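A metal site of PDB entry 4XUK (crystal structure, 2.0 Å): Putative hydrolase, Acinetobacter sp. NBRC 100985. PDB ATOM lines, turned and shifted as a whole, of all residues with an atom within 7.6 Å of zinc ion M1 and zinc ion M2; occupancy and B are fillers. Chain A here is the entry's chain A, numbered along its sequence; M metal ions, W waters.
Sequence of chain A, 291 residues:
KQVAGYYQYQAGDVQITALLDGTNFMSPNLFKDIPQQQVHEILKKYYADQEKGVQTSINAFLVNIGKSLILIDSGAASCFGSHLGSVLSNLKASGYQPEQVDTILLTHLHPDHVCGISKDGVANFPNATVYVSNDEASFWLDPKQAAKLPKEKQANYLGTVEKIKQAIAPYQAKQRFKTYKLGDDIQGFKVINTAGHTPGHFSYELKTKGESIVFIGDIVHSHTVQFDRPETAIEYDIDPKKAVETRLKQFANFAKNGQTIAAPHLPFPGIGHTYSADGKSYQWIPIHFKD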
ATOM      1  N   SER A  57      24.300 -19.723   8.940  1.00  0.00           N
ATOM      2  CA  SER A  57      24.743 -18.646   8.071  1.00  0.00           C
ATOM      3  C   SER A  57      25.264 -17.470   8.896  1.00  0.00           C
ATOM      4  O   SER A  57      24.901 -17.288  10.065  1.00  0.00           O
ATOM      5  CB  SER A  57      23.594 -18.172   7.177  1.00  0.00           C
ATOM      6  OG  SER A  57      23.136 -19.192   6.320  1.00  0.00           O
ATOM      7  N   ILE A  58      26.130 -16.677   8.265  1.00  0.00           N
ATOM      8  CA  ILE A  58      26.505 -15.386   8.795  1.00  0.00           C
ATOM      9  C   ILE A  58      26.199 -14.409   7.673  1.00  0.00           C
ATOM     10  O   ILE A  58      26.804 -14.470   6.606  1.00  0.00           O
ATOM     11  CB  ILE A  58      28.008 -15.312   9.164  1.00  0.00           C
ATOM     12  CG1 ILE A  58      28.385 -16.355  10.215  1.00  0.00           C
ATOM     13  CG2 ILE A  58      28.347 -13.911   9.716  1.00  0.00           C
ATOM     14  CD1 ILE A  58      28.723 -17.725   9.633  1.00  0.00           C
ATOM     15  N   ASN A  59      25.226 -13.533   7.902  1.00  0.00           N
ATOM     16  CA  ASN A  59      24.782 -12.591   6.885  1.00  0.00           C
ATOM     17  C   ASN A  59      25.006 -11.127   7.311  1.00  0.00           C
ATOM     18  O   ASN A  59      25.190 -10.824   8.512  1.00  0.00           O
ATOM     19  CB  ASN A  59      23.298 -12.783   6.573  1.00  0.00           C
ATOM     20  CG  ASN A  59      22.905 -14.241   6.392  1.00  0.00           C
ATOM     21  OD1 ASN A  59      23.527 -14.984   5.636  1.00  0.00           O
ATOM     22  ND2 ASN A  59      21.848 -14.645   7.071  1.00  0.00           N
ATOM     23  N   ASP A  73      25.547  -4.527   9.970  1.00  0.00           N
ATOM     24  CA  ASP A  73      26.598  -5.530  10.182  1.00  0.00           C
ATOM     25  C   ASP A  73      27.440  -5.753   8.912  1.00  0.00           C
ATOM     26  O   ASP A  73      27.075  -5.280   7.839  1.00  0.00           O
ATOM     27  CB  ASP A  73      26.037  -6.841  10.787  1.00  0.00           C
ATOM     28  CG  ASP A  73      25.518  -6.637  12.194  1.00  0.00           C
ATOM     29  OD1 ASP A  73      25.906  -5.613  12.818  1.00  0.00           O
ATOM     30  OD2 ASP A  73      24.715  -7.470  12.678  1.00  0.00           O
ATOM     31  N   PHE A  80      37.964 -14.555  11.849  1.00  0.00           N
ATOM     32  CA  PHE A  80      37.576 -15.910  12.278  1.00  0.00           C
ATOM     33  C   PHE A  80      38.034 -16.960  11.304  1.00  0.00           C
ATOM     34  O   PHE A  80      37.490 -18.070  11.262  1.00  0.00           O
ATOM     35  CB  PHE A  80      36.050 -16.019  12.446  1.00  0.00           C
ATOM     36  CG  PHE A  80      35.550 -15.530  13.778  1.00  0.00           C
ATOM     37  CD1 PHE A  80      36.343 -15.631  14.915  1.00  0.00           C
ATOM     38  CD2 PHE A  80      34.281 -14.976  13.890  1.00  0.00           C
ATOM     39  CE1 PHE A  80      35.871 -15.185  16.142  1.00  0.00           C
ATOM     40  CE2 PHE A  80      33.806 -14.539  15.120  1.00  0.00           C
ATOM     41  CZ  PHE A  80      34.608 -14.636  16.242  1.00  0.00           C
ATOM     42  N   THR A 107      24.854  -4.168  15.072  1.00  0.00           N
ATOM     43  CA  THR A 107      23.954  -4.664  16.112  1.00  0.00           C
ATOM     44  C   THR A 107      24.719  -4.868  17.410  1.00  0.00           C
ATOM     45  O   THR A 107      24.175  -4.626  18.502  1.00  0.00           O
ATOM     46  CB  THR A 107      23.259  -5.971  15.703  1.00  0.00           C
ATOM     47  OG1 THR A 107      24.247  -6.955  15.351  1.00  0.00           O
ATOM     48  CG2 THR A 107      22.323  -5.716  14.527  1.00  0.00           C
ATOM     49  N   HIS A 108      25.972  -5.284  17.279  1.00  0.00           N
ATOM     50  CA  HIS A 108      26.889  -5.462  18.405  1.00  0.00           C
ATOM     51  C   HIS A 108      28.305  -5.625  17.872  1.00  0.00           C
ATOM     52  O   HIS A 108      28.513  -5.684  16.651  1.00  0.00           O
ATOM     53  CB  HIS A 108      26.509  -6.666  19.300  1.00  0.00           C
ATOM     54  CG  HIS A 108      26.427  -7.975  18.568  1.00  0.00           C
ATOM     55  ND1 HIS A 108      25.736  -8.134  17.385  1.00  0.00           N
ATOM     56  CD2 HIS A 108      26.924  -9.191  18.892  1.00  0.00           C
ATOM     57  CE1 HIS A 108      25.829  -9.395  16.997  1.00  0.00           C
ATOM     58  NE2 HIS A 108      26.538 -10.051  17.893  1.00  0.00           N
ATOM     59  N   LEU A 109      29.282  -5.724  18.770  1.00  0.00           N
ATOM     60  CA  LEU A 109      30.684  -5.706  18.357  1.00  0.00           C
ATOM     61  C   LEU A 109      31.362  -7.085  18.324  1.00  0.00           C
ATOM     62  O   LEU A 109      32.585  -7.153  18.289  1.00  0.00           O
ATOM     63  CB  LEU A 109      31.484  -4.744  19.248  1.00  0.00           C
ATOM     64  CG  LEU A 109      31.108  -3.262  19.150  1.00  0.00           C
ATOM     65  CD1 LEU A 109      31.858  -2.440  20.204  1.00  0.00           C
ATOM     66  CD2 LEU A 109      31.433  -2.731  17.776  1.00  0.00           C
ATOM     67  N   HIS A 110      30.586  -8.172  18.308  1.00  0.00           N
ATOM     68  CA  HIS A 110      31.185  -9.486  18.065  1.00  0.00           C
ATOM     69  C   HIS A 110      31.892  -9.421  16.699  1.00  0.00           C
ATOM     70  O   HIS A 110      31.421  -8.745  15.787  1.00  0.00           O
ATOM     71  CB  HIS A 110      30.134 -10.628  18.144  1.00  0.00           C
ATOM     72  CG  HIS A 110      29.984 -11.191  19.529  1.00  0.00           C
ATOM     73  ND1 HIS A 110      28.903 -11.946  19.907  1.00  0.00           N
ATOM     74  CD2 HIS A 110      30.789 -11.115  20.621  1.00  0.00           C
ATOM     75  CE1 HIS A 110      29.026 -12.301  21.172  1.00  0.00           C
ATOM     76  NE2 HIS A 110      30.165 -11.805  21.631  1.00  0.00           N
ATOM     77  N   PRO A 111      33.046 -10.097  16.575  1.00  0.00           N
ATOM     78  CA  PRO A 111      33.864  -9.983  15.359  1.00  0.00           C
ATOM     79  C   PRO A 111      33.157 -10.355  14.060  1.00  0.00           C
ATOM     80  O   PRO A 111      33.524  -9.819  13.020  1.00  0.00           O
ATOM     81  CB  PRO A 111      35.011 -10.963  15.636  1.00  0.00           C
ATOM     82  CG  PRO A 111      35.154 -10.913  17.153  1.00  0.00           C
ATOM     83  CD  PRO A 111      33.728 -10.854  17.643  1.00  0.00           C
ATOM     84  N   ASP A 112      32.157 -11.241  14.113  1.00  0.00           N
ATOM     85  CA  ASP A 112      31.482 -11.627  12.881  1.00  0.00           C
ATOM     86  C   ASP A 112      30.438 -10.583  12.450  1.00  0.00           C
ATOM     87  O   ASP A 112      29.686 -10.796  11.503  1.00  0.00           O
ATOM     88  CB  ASP A 112      30.858 -13.023  13.023  1.00  0.00           C
ATOM     89  CG  ASP A 112      29.964 -13.139  14.239  1.00  0.00           C
ATOM     90  OD1 ASP A 112      30.357 -12.663  15.322  1.00  0.00           O
ATOM     91  OD2 ASP A 112      28.873 -13.707  14.105  1.00  0.00           O
ATOM     92  N   HIS A 113      30.425  -9.450  13.142  1.00  0.00           N
ATOM     93  CA  HIS A 113      29.560  -8.345  12.758  1.00  0.00           C
ATOM     94  C   HIS A 113      30.331  -7.072  12.481  1.00  0.00           C
ATOM     95  O   HIS A 113      29.954  -6.303  11.570  1.00  0.00           O
ATOM     96  CB  HIS A 113      28.505  -8.132  13.846  1.00  0.00           C
ATOM     97  CG  HIS A 113      27.692  -9.356  14.105  1.00  0.00           C
ATOM     98  ND1 HIS A 113      26.424  -9.518  13.614  1.00  0.00           N
ATOM     99  CD2 HIS A 113      28.012 -10.520  14.720  1.00  0.00           C
ATOM    100  CE1 HIS A 113      25.978 -10.713  13.948  1.00  0.00           C
ATOM    101  NE2 HIS A 113      26.916 -11.341  14.631  1.00  0.00           N
ATOM    102  N   GLU A 136      27.182  -0.827  24.235  1.00  0.00           N
ATOM    103  CA  GLU A 136      27.994  -1.867  23.595  1.00  0.00           C
ATOM    104  C   GLU A 136      29.457  -1.458  23.550  1.00  0.00           C
ATOM    105  O   GLU A 136      30.339  -2.246  23.908  1.00  0.00           O
ATOM    106  CB  GLU A 136      27.476  -2.175  22.191  1.00  0.00           C
ATOM    107  CG  GLU A 136      28.241  -3.283  21.480  1.00  0.00           C
ATOM    108  CD  GLU A 136      27.939  -4.677  22.019  1.00  0.00           C
ATOM    109  OE1 GLU A 136      27.032  -4.815  22.864  1.00  0.00           O
ATOM    110  OE2 GLU A 136      28.590  -5.641  21.566  1.00  0.00           O
ATOM    111  N   HIS A 197      22.477 -10.982  24.626  1.00  0.00           N
ATOM    112  CA  HIS A 197      23.533 -11.611  23.839  1.00  0.00           C
ATOM    113  C   HIS A 197      24.862 -10.900  24.073  1.00  0.00           C
ATOM    114  O   HIS A 197      25.898 -11.539  24.238  1.00  0.00           O
ATOM    115  CB  HIS A 197      23.181 -11.576  22.364  1.00  0.00           C
ATOM    116  CG  HIS A 197      24.224 -12.181  21.482  1.00  0.00           C
ATOM    117  ND1 HIS A 197      24.555 -13.520  21.515  1.00  0.00           N
ATOM    118  CD2 HIS A 197      25.001 -11.624  20.527  1.00  0.00           C
ATOM    119  CE1 HIS A 197      25.496 -13.753  20.618  1.00  0.00           C
ATOM    120  NE2 HIS A 197      25.778 -12.616  20.003  1.00  0.00           N
ATOM    121  N   THR A 198      24.826  -9.565  24.077  1.00  0.00           N
ATOM    122  CA  THR A 198      25.935  -8.745  24.573  1.00  0.00           C
ATOM    123  C   THR A 198      25.299  -7.628  25.373  1.00  0.00           C
ATOM    124  O   THR A 198      24.117  -7.347  25.193  1.00  0.00           O
ATOM    125  CB  THR A 198      26.777  -8.121  23.431  1.00  0.00           C
ATOM    126  OG1 THR A 198      25.995  -7.170  22.715  1.00  0.00           O
ATOM    127  CG2 THR A 198      27.318  -9.197  22.481  1.00  0.00           C
ATOM    128  N   HIS A 201      23.660  -5.023  22.938  1.00  0.00           N
ATOM    129  CA  HIS A 201      23.098  -5.508  21.682  1.00  0.00           C
ATOM    130  C   HIS A 201      21.835  -4.732  21.356  1.00  0.00           C
ATOM    131  O   HIS A 201      20.953  -4.588  22.209  1.00  0.00           O
ATOM    132  CB  HIS A 201      22.792  -7.002  21.755  1.00  0.00           C
ATOM    133  CG  HIS A 201      22.414  -7.611  20.439  1.00  0.00           C
ATOM    134  ND1 HIS A 201      21.155  -7.510  19.911  1.00  0.00           N
ATOM    135  CD2 HIS A 201      23.145  -8.320  19.543  1.00  0.00           C
ATOM    136  CE1 HIS A 201      21.115  -8.137  18.748  1.00  0.00           C
ATOM    137  NE2 HIS A 201      22.321  -8.624  18.495  1.00  0.00           N
ATOM    138  N   GLY A 217      19.659  -8.709  14.483  1.00  0.00           N
ATOM    139  CA  GLY A 217      20.944  -9.063  15.047  1.00  0.00           C
ATOM    140  C   GLY A 217      20.907 -10.469  15.642  1.00  0.00           C
ATOM    141  O   GLY A 217      20.195 -11.349  15.144  1.00  0.00           O
ATOM    142  N   ASP A 218      21.664 -10.673  16.711  1.00  0.00           N
ATOM    143  CA  ASP A 218      21.874 -12.005  17.258  1.00  0.00           C
ATOM    144  C   ASP A 218      20.984 -12.363  18.441  1.00  0.00           C
ATOM    145  O   ASP A 218      21.453 -12.926  19.428  1.00  0.00           O
ATOM    146  CB  ASP A 218      23.338 -12.164  17.677  1.00  0.00           C
ATOM    147  CG  ASP A 218      24.254 -12.383  16.502  1.00  0.00           C
ATOM    148  OD1 ASP A 218      23.833 -12.138  15.346  1.00  0.00           O
ATOM    149  OD2 ASP A 218      25.378 -12.851  16.729  1.00  0.00           O
ATOM    150  N   ILE A 219      19.696 -12.067  18.339  1.00  0.00           N
ATOM    151  CA  ILE A 219      18.747 -12.527  19.345  1.00  0.00           C
ATOM    152  C   ILE A 219      18.372 -13.976  19.041  1.00  0.00           C
ATOM    153  O   ILE A 219      17.574 -14.583  19.769  1.00  0.00           O
ATOM    154  CB  ILE A 219      17.489 -11.668  19.371  1.00  0.00           C
ATOM    155  CG1 ILE A 219      16.765 -11.742  18.015  1.00  0.00           C
ATOM    156  CG2 ILE A 219      17.849 -10.209  19.697  1.00  0.00           C
ATOM    157  CD1 ILE A 219      15.434 -11.023  18.000  1.00  0.00           C
ATOM    158  N   VAL A 220      18.943 -14.526  17.973  1.00  0.00           N
ATOM    159  CA  VAL A 220      18.733 -15.940  17.640  1.00  0.00           C
ATOM    160  C   VAL A 220      19.833 -16.474  16.720  1.00  0.00           C
ATOM    161  O   VAL A 220      20.395 -15.734  15.897  1.00  0.00           O
ATOM    162  CB  VAL A 220      17.306 -16.161  17.044  1.00  0.00           C
ATOM    163  CG1 VAL A 220      17.239 -15.755  15.566  1.00  0.00           C
ATOM    164  CG2 VAL A 220      16.895 -17.616  17.213  1.00  0.00           C
ATOM    165  N   HIS A 221      20.163 -17.762  16.871  1.00  0.00           N
ATOM    166  CA  HIS A 221      21.265 -18.373  16.121  1.00  0.00           C
ATOM    167  C   HIS A 221      20.871 -19.583  15.288  1.00  0.00           C
ATOM    168  O   HIS A 221      21.739 -20.281  14.763  1.00  0.00           O
ATOM    169  CB  HIS A 221      22.388 -18.763  17.070  1.00  0.00           C
ATOM    170  CG  HIS A 221      23.201 -17.615  17.558  1.00  0.00           C
ATOM    171  ND1 HIS A 221      22.687 -16.640  18.382  1.00  0.00           N
ATOM    172  CD2 HIS A 221      24.485 -17.254  17.298  1.00  0.00           C
ATOM    173  CE1 HIS A 221      23.617 -15.739  18.629  1.00  0.00           C
ATOM    174  NE2 HIS A 221      24.715 -16.090  17.983  1.00  0.00           N
ATOM    175  N   TYR A 236      27.163 -18.605  23.123  1.00  0.00           N
ATOM    176  CA  TYR A 236      27.650 -17.300  22.676  1.00  0.00           C
ATOM    177  C   TYR A 236      27.062 -16.116  23.452  1.00  0.00           C
ATOM    178  O   TYR A 236      27.645 -15.017  23.444  1.00  0.00           O
ATOM    179  CB  TYR A 236      27.362 -17.100  21.166  1.00  0.00           C
ATOM    180  CG  TYR A 236      27.963 -18.141  20.246  1.00  0.00           C
ATOM    181  CD1 TYR A 236      29.253 -18.629  20.433  1.00  0.00           C
ATOM    182  CD2 TYR A 236      27.233 -18.644  19.175  1.00  0.00           C
ATOM    183  CE1 TYR A 236      29.791 -19.583  19.589  1.00  0.00           C
ATOM    184  CE2 TYR A 236      27.768 -19.600  18.322  1.00  0.00           C
ATOM    185  CZ  TYR A 236      29.042 -20.056  18.538  1.00  0.00           C
ATOM    186  OH  TYR A 236      29.582 -21.001  17.692  1.00  0.00           O
ATOM    187  N   ASP A 237      25.905 -16.318  24.071  1.00  0.00           N
ATOM    188  CA  ASP A 237      25.256 -15.257  24.843  1.00  0.00           C
ATOM    189  C   ASP A 237      26.124 -14.893  26.058  1.00  0.00           C
ATOM    190  O   ASP A 237      26.568 -15.774  26.791  1.00  0.00           O
ATOM    191  CB  ASP A 237      23.877 -15.708  25.333  1.00  0.00           C
ATOM    192  CG  ASP A 237      22.881 -15.891  24.206  1.00  0.00           C
ATOM    193  OD1 ASP A 237      23.059 -15.282  23.131  1.00  0.00           O
ATOM    194  OD2 ASP A 237      21.904 -16.656  24.389  1.00  0.00           O
ATOM    195  N   PRO A 264      21.175 -11.937  10.896  1.00  0.00           N
ATOM    196  CA  PRO A 264      22.503 -12.357  10.473  1.00  0.00           C
ATOM    197  C   PRO A 264      22.740 -13.868  10.613  1.00  0.00           C
ATOM    198  O   PRO A 264      23.587 -14.387   9.885  1.00  0.00           O
ATOM    199  CB  PRO A 264      23.439 -11.579  11.411  1.00  0.00           C
ATOM    200  CG  PRO A 264      22.618 -11.272  12.609  1.00  0.00           C
ATOM    201  CD  PRO A 264      21.223 -11.045  12.065  1.00  0.00           C
ATOM    202  N   HIS A 265      22.020 -14.550  11.511  1.00  0.00           N
ATOM    203  CA  HIS A 265      22.247 -15.985  11.693  1.00  0.00           C
ATOM    204  C   HIS A 265      21.081 -16.923  11.348  1.00  0.00           C
ATOM    205  O   HIS A 265      21.022 -18.034  11.868  1.00  0.00           O
ATOM    206  CB  HIS A 265      22.716 -16.271  13.126  1.00  0.00           C
ATOM    207  CG  HIS A 265      24.061 -15.696  13.432  1.00  0.00           C
ATOM    208  ND1 HIS A 265      25.101 -15.743  12.530  1.00  0.00           N
ATOM    209  CD2 HIS A 265      24.539 -15.058  14.528  1.00  0.00           C
ATOM    210  CE1 HIS A 265      26.158 -15.147  13.056  1.00  0.00           C
ATOM    211  NE2 HIS A 265      25.844 -14.734  14.268  1.00  0.00           N
HETATM  212 ZN    ZN M   1      27.101 -12.242  18.333  1.00  0.00          ZN
HETATM  213 ZN    ZN M   2      26.997 -13.205  15.387  1.00  0.00          ZN
HETATM  214  O   HOH W   1      27.524 -15.141  18.050  1.00  0.00           O
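ND1 of His 113 sits at hydrogen-bond distance from OD2 of Asp 73 (2.8 Å). A ring nitrogen (NE2) of His 201 is in hydrogen-bond range of the backbone NH (N) of Asp 218, at 2.8 Å. A ring nitrogen (ND1) of His 197 sits at hydrogen-bond distance from the side-chain carboxylate (OD1) of Asp 237 (2.8 Å). ND1 of His 265 is in hydrogen-bond range of O of Ser 57. A ring nitrogen (ND1) of His 108 sits at hydrogen-bond distance from the side-chain hydroxyl (OG1) of Thr 107 (2.8 Å).
Of the 25 residues printed, 5 come within 4 Å of zinc ion M1. The nearest printed residue that does not touch zinc ion M1 is Asp 112 (4.5 Å).
Four residues have an atom within 4 Å of zinc ion M2: Asp 112, His 113, Asp 218 and His 265. The nearest printed residue that does not touch zinc ion M2 is His 108 (4.1 Å).
Zinc ion M1 is bound by NE2 of His 197 (2.2 Å), NE2 of His 108 (2.3 Å), ND1 of His 110 (2.4 Å) and OD2 of Asp 218 (2.4 Å).
Zinc ion M2 is bound by NE2 of His 113, OD2 of Asp 218, NE2 of His 265 and OD2 of Asp 112. Zinc ion M2 has four donor atoms within binding distance.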
